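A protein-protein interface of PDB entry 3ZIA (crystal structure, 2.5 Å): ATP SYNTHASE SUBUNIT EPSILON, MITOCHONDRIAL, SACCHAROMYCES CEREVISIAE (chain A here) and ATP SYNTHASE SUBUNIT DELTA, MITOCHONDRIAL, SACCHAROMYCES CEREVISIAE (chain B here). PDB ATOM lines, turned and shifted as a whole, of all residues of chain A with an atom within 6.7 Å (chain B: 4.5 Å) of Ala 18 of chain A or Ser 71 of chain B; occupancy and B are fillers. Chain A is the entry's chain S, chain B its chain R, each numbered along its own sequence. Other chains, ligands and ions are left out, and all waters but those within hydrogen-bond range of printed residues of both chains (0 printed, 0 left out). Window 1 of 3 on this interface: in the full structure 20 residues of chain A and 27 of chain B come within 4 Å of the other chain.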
ATOM      1  N   TYR A  13     -15.785  -7.869 -19.689  1.00  0.00           N
ATOM      2  CA  TYR A  13     -15.200  -7.319 -20.906  1.00  0.00           C
ATOM      3  C   TYR A  13     -15.269  -5.786 -20.927  1.00  0.00           C
ATOM      4  O   TYR A  13     -14.250  -5.115 -21.161  1.00  0.00           O
ATOM      5  CB  TYR A  13     -15.877  -7.939 -22.143  1.00  0.00           C
ATOM      6  CG  TYR A  13     -15.959  -7.039 -23.363  1.00  0.00           C
ATOM      7  CD1 TYR A  13     -14.820  -6.759 -24.133  1.00  0.00           C
ATOM      8  CD2 TYR A  13     -17.175  -6.477 -23.755  1.00  0.00           C
ATOM      9  CE1 TYR A  13     -14.889  -5.923 -25.253  1.00  0.00           C
ATOM     10  CE2 TYR A  13     -17.259  -5.646 -24.876  1.00  0.00           C
ATOM     11  CZ  TYR A  13     -16.113  -5.375 -25.619  1.00  0.00           C
ATOM     12  OH  TYR A  13     -16.193  -4.558 -26.723  1.00  0.00           O
ATOM     13  N   LEU A  14     -16.459  -5.243 -20.674  1.00  0.00           N
ATOM     14  CA  LEU A  14     -16.673  -3.796 -20.684  1.00  0.00           C
ATOM     15  C   LEU A  14     -15.820  -3.082 -19.643  1.00  0.00           C
ATOM     16  O   LEU A  14     -15.347  -1.966 -19.866  1.00  0.00           O
ATOM     17  CB  LEU A  14     -18.140  -3.475 -20.435  1.00  0.00           C
ATOM     18  CG  LEU A  14     -19.154  -3.948 -21.468  1.00  0.00           C
ATOM     19  CD1 LEU A  14     -20.543  -3.826 -20.887  1.00  0.00           C
ATOM     20  CD2 LEU A  14     -19.024  -3.148 -22.758  1.00  0.00           C
ATOM     21  N   ASN A  15     -15.638  -3.733 -18.501  1.00  0.00           N
ATOM     22  CA  ASN A  15     -14.817  -3.195 -17.431  1.00  0.00           C
ATOM     23  C   ASN A  15     -13.350  -3.101 -17.842  1.00  0.00           C
ATOM     24  O   ASN A  15     -12.731  -2.043 -17.690  1.00  0.00           O
ATOM     25  CB  ASN A  15     -14.967  -4.042 -16.171  1.00  0.00           C
ATOM     26  CG  ASN A  15     -13.980  -3.657 -15.097  1.00  0.00           C
ATOM     27  OD1 ASN A  15     -13.147  -4.468 -14.695  1.00  0.00           O
ATOM     28  ND2 ASN A  15     -14.052  -2.407 -14.640  1.00  0.00           N
ATOM     29  N   VAL A  16     -12.810  -4.209 -18.356  1.00  0.00           N
ATOM     30  CA  VAL A  16     -11.467  -4.246 -18.953  1.00  0.00           C
ATOM     31  C   VAL A  16     -11.253  -3.046 -19.888  1.00  0.00           C
ATOM     32  O   VAL A  16     -10.239  -2.339 -19.786  1.00  0.00           O
ATOM     33  CB  VAL A  16     -11.210  -5.589 -19.684  1.00  0.00           C
ATOM     34  CG1 VAL A  16     -10.029  -5.482 -20.640  1.00  0.00           C
ATOM     35  CG2 VAL A  16     -10.971  -6.702 -18.677  1.00  0.00           C
ATOM     36  N   ALA A  17     -12.228  -2.810 -20.766  1.00  0.00           N
ATOM     37  CA  ALA A  17     -12.237  -1.637 -21.636  1.00  0.00           C
ATOM     38  C   ALA A  17     -12.225  -0.355 -20.818  1.00  0.00           C
ATOM     39  O   ALA A  17     -11.290   0.445 -20.926  1.00  0.00           O
ATOM     40  CB  ALA A  17     -13.451  -1.663 -22.564  1.00  0.00           C
ATOM     41  N   ALA A  18     -13.260  -0.180 -19.994  1.00  0.00           N
ATOM     42  CA  ALA A  18     -13.454   1.022 -19.172  1.00  0.00           C
ATOM     43  C   ALA A  18     -12.205   1.405 -18.381  1.00  0.00           C
ATOM     44  O   ALA A  18     -11.876   2.587 -18.272  1.00  0.00           O
ATOM     45  CB  ALA A  18     -14.636   0.839 -18.240  1.00  0.00           C
ATOM     46  N   GLN A  19     -11.520   0.395 -17.842  1.00  0.00           N
ATOM     47  CA  GLN A  19     -10.218   0.568 -17.200  1.00  0.00           C
ATOM     48  C   GLN A  19      -9.208   1.254 -18.118  1.00  0.00           C
ATOM     49  O   GLN A  19      -8.690   2.330 -17.790  1.00  0.00           O
ATOM     50  CB  GLN A  19      -9.669  -0.783 -16.730  1.00  0.00           C
ATOM     51  CG  GLN A  19      -9.738  -0.992 -15.233  1.00  0.00           C
ATOM     52  CD  GLN A  19      -8.644  -0.241 -14.501  1.00  0.00           C
ATOM     53  OE1 GLN A  19      -7.536  -0.748 -14.336  1.00  0.00           O
ATOM     54  NE2 GLN A  19      -8.947   0.974 -14.063  1.00  0.00           N
ATOM     55  N   ALA A  20      -8.946   0.635 -19.269  1.00  0.00           N
ATOM     56  CA  ALA A  20      -8.023   1.181 -20.256  1.00  0.00           C
ATOM     57  C   ALA A  20      -8.353   2.637 -20.609  1.00  0.00           C
ATOM     58  O   ALA A  20      -7.454   3.471 -20.744  1.00  0.00           O
ATOM     59  CB  ALA A  20      -8.011   0.315 -21.495  1.00  0.00           C
ATOM     60  N   ILE A  21      -9.643   2.934 -20.739  1.00  0.00           N
ATOM     61  CA  ILE A  21     -10.117   4.288 -21.047  1.00  0.00           C
ATOM     62  C   ILE A  21      -9.855   5.277 -19.908  1.00  0.00           C
ATOM     63  O   ILE A  21      -9.536   6.440 -20.159  1.00  0.00           O
ATOM     64  CB  ILE A  21     -11.612   4.274 -21.414  1.00  0.00           C
ATOM     65  CG1 ILE A  21     -11.830   3.312 -22.577  1.00  0.00           C
ATOM     66  CG2 ILE A  21     -12.106   5.679 -21.775  1.00  0.00           C
ATOM     67  CD1 ILE A  21     -13.103   2.558 -22.513  1.00  0.00           C
ATOM     68  N   ARG A  22      -9.985   4.811 -18.666  1.00  0.00           N
ATOM     69  CA  ARG A  22      -9.682   5.640 -17.496  1.00  0.00           C
ATOM     70  C   ARG A  22      -8.180   5.912 -17.395  1.00  0.00           C
ATOM     71  O   ARG A  22      -7.763   7.062 -17.235  1.00  0.00           O
ATOM     72  CB  ARG A  22     -10.209   5.001 -16.204  1.00  0.00           C
ATOM     73  CG  ARG A  22     -11.725   5.073 -16.027  1.00  0.00           C
ATOM     74  CD  ARG A  22     -12.162   4.610 -14.646  1.00  0.00           C
ATOM     75  NE  ARG A  22     -11.920   3.189 -14.381  1.00  0.00           N
ATOM     76  CZ  ARG A  22     -12.790   2.212 -14.634  1.00  0.00           C
ATOM     77  NH1 ARG A  22     -13.972   2.494 -15.182  1.00  0.00           N
ATOM     78  NH2 ARG A  22     -12.484   0.946 -14.339  1.00  0.00           N
ATOM     79  N   SER A  23      -7.374   4.853 -17.508  1.00  0.00           N
ATOM     80  CA  SER A  23      -5.912   4.979 -17.543  1.00  0.00           C
ATOM     81  C   SER A  23      -5.426   5.856 -18.707  1.00  0.00           C
ATOM     82  O   SER A  23      -4.337   6.436 -18.638  1.00  0.00           O
ATOM     83  CB  SER A  23      -5.247   3.603 -17.629  1.00  0.00           C
ATOM     84  OG  SER A  23      -5.624   2.761 -16.558  1.00  0.00           O
ATOM     85  N   SER A  38     -11.353   2.440 -10.165  1.00  0.00           N
ATOM     86  CA  SER A  38     -10.378   1.508 -10.736  1.00  0.00           C
ATOM     87  C   SER A  38      -9.838   0.459  -9.757  1.00  0.00           C
ATOM     88  O   SER A  38      -9.262  -0.544 -10.182  1.00  0.00           O
ATOM     89  CB  SER A  38      -9.204   2.292 -11.326  1.00  0.00           C
ATOM     90  OG  SER A  38      -9.651   3.284 -12.234  1.00  0.00           O
ATOM     91  N   PRO B  54     -17.055  -0.547 -27.949  1.00  0.00           N
ATOM     92  CA  PRO B  54     -16.293   0.630 -27.545  1.00  0.00           C
ATOM     93  C   PRO B  54     -15.947   1.495 -28.755  1.00  0.00           C
ATOM     94  O   PRO B  54     -15.153   1.093 -29.609  1.00  0.00           O
ATOM     95  CB  PRO B  54     -15.032   0.035 -26.913  1.00  0.00           C
ATOM     96  CG  PRO B  54     -14.921  -1.335 -27.487  1.00  0.00           C
ATOM     97  CD  PRO B  54     -16.318  -1.798 -27.699  1.00  0.00           C
ATOM     98  N   ILE B  70     -16.881   6.422 -25.614  1.00  0.00           N
ATOM     99  CA  ILE B  70     -17.442   5.579 -24.558  1.00  0.00           C
ATOM    100  C   ILE B  70     -16.714   4.244 -24.401  1.00  0.00           C
ATOM    101  O   ILE B  70     -15.824   3.917 -25.185  1.00  0.00           O
ATOM    102  CB  ILE B  70     -18.965   5.340 -24.749  1.00  0.00           C
ATOM    103  CG1 ILE B  70     -19.233   4.354 -25.896  1.00  0.00           C
ATOM    104  CG2 ILE B  70     -19.691   6.671 -24.952  1.00  0.00           C
ATOM    105  CD1 ILE B  70     -20.589   3.668 -25.826  1.00  0.00           C
ATOM    106  N   SER B  71     -17.102   3.488 -23.377  1.00  0.00           N
ATOM    107  CA  SER B  71     -16.521   2.183 -23.087  1.00  0.00           C
ATOM    108  C   SER B  71     -17.310   1.059 -23.730  1.00  0.00           C
ATOM    109  O   SER B  71     -16.805  -0.054 -23.882  1.00  0.00           O
ATOM    110  CB  SER B  71     -16.470   1.955 -21.576  1.00  0.00           C
ATOM    111  OG  SER B  71     -17.766   2.005 -21.012  1.00  0.00           O
ATOM    112  N   GLY B  72     -18.553   1.356 -24.093  1.00  0.00           N
ATOM    113  CA  GLY B  72     -19.476   0.354 -24.606  1.00  0.00           C
ATOM    114  C   GLY B  72     -20.561   0.020 -23.601  1.00  0.00           C
ATOM    115  O   GLY B  72     -20.321   0.019 -22.393  1.00  0.00           O
ATOM    116  N   ALA B  87     -23.595   3.705 -20.753  1.00  0.00           N
ATOM    117  CA  ALA B  87     -22.192   3.300 -20.837  1.00  0.00           C
ATOM    118  C   ALA B  87     -21.497   3.477 -19.495  1.00  0.00           C
ATOM    119  O   ALA B  87     -21.842   4.375 -18.729  1.00  0.00           O
ATOM    120  CB  ALA B  87     -21.470   4.091 -21.917  1.00  0.00           C
ATOM    121  N   ILE B  88     -20.517   2.618 -19.228  1.00  0.00           N
ATOM    122  CA  ILE B  88     -19.733   2.663 -17.994  1.00  0.00           C
ATOM    123  C   ILE B  88     -18.833   3.899 -17.937  1.00  0.00           C
ATOM    124  O   ILE B  88     -18.887   4.663 -16.974  1.00  0.00           O
ATOM    125  CB  ILE B  88     -18.919   1.372 -17.815  1.00  0.00           C
ATOM    126  CG1 ILE B  88     -19.871   0.187 -17.702  1.00  0.00           C
ATOM    127  CG2 ILE B  88     -18.037   1.445 -16.582  1.00  0.00           C
ATOM    128  CD1 ILE B  88     -19.517  -0.935 -18.618  1.00  0.00           C
ATOM    129  N   GLU B  89     -18.012   4.092 -18.964  1.00  0.00           N
ATOM    130  CA  GLU B  89     -17.218   5.313 -19.088  1.00  0.00           C
ATOM    131  C   GLU B  89     -17.545   6.054 -20.376  1.00  0.00           C
ATOM    132  O   GLU B  89     -17.879   5.438 -21.389  1.00  0.00           O
ATOM    133  CB  GLU B  89     -15.717   5.011 -19.034  1.00  0.00           C
ATOM    134  CG  GLU B  89     -15.215   4.469 -17.703  1.00  0.00           C
ATOM    135  CD  GLU B  89     -15.334   5.453 -16.544  1.00  0.00           C
ATOM    136  OE1 GLU B  89     -15.589   6.661 -16.764  1.00  0.00           O
ATOM    137  OE2 GLU B  89     -15.168   5.002 -15.396  1.00  0.00           O
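N of Ser 71 of chain B sits at hydrogen-bond distance from O of Glu 89 of chain B (2.9 Å).
OG of Ser 71 of chain B lies within hydrogen-bond range of N of Ile 88 of chain B.
The guanidinium group (NE) of Arg 22 of chain A lies within hydrogen-bond range of the side-chain hydroxyl (OG) of Ser 38 of chain A, at 3.1 Å.
Among the printed residues, pairs that only touch across the chains: Tyr 13 of chain A with Pro 54 of chain B, Leu 14 of chain A with Ile 88 of chain B, Leu 14 of chain A with Gly 72 of chain B, Ile 21 of chain A with Ser 71 of chain B, Ala 18 of chain A with Glu 89 of chain B, Ala 18 of chain A with Ile 88 of chain B, Ala 17 of chain A with Ser 71 of chain B, Ala 18 of chain A with Ser 71 of chain B and Leu 14 of chain A with Ser 71 of chain B.
Ala 20 of chain A touches none of the printed residues of chain B.
Of the printed residues of chain A, Pro 54 of chain B touches Tyr 13.
Of chain A, only Leu 14 (3.97 Å), Ala 17 (3.9 Å), Ala 18 (3.97 Å) and Ile 21 (3.5 Å) come within 4 Å of Ser 71 of chain B.
Of the printed residues of chain A, Gly 72 of chain B touches Leu 14 (3.4 Å).
Ala 87 of chain B touches none of the printed residues of chain A.
Of the printed residues of chain A, Ile 88 of chain B touches Leu 14 (3.4 Å) and Ala 18 (3.8 Å).
The nearest residue of chain A that does not touch Ser 71 of chain B is Tyr 13 of chain A (5.4 Å).
Hydrophobic or aromatic side chains of chain A that line the printed part of chain B: Tyr 13, Leu 14, Ala 17, Ala 18 and Ile 21.
Among the printed residues, Asp or Glu carboxylates within 4 Å of a Lys or Arg side-chain nitrogen of the other chain: Arg 22 of chain A with Glu 89 of chain B (2.8 Å).
OE2 of Glu 89 of chain B is in salt-bridge range of NH1 of Arg 22 of chain A (2.8 Å).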
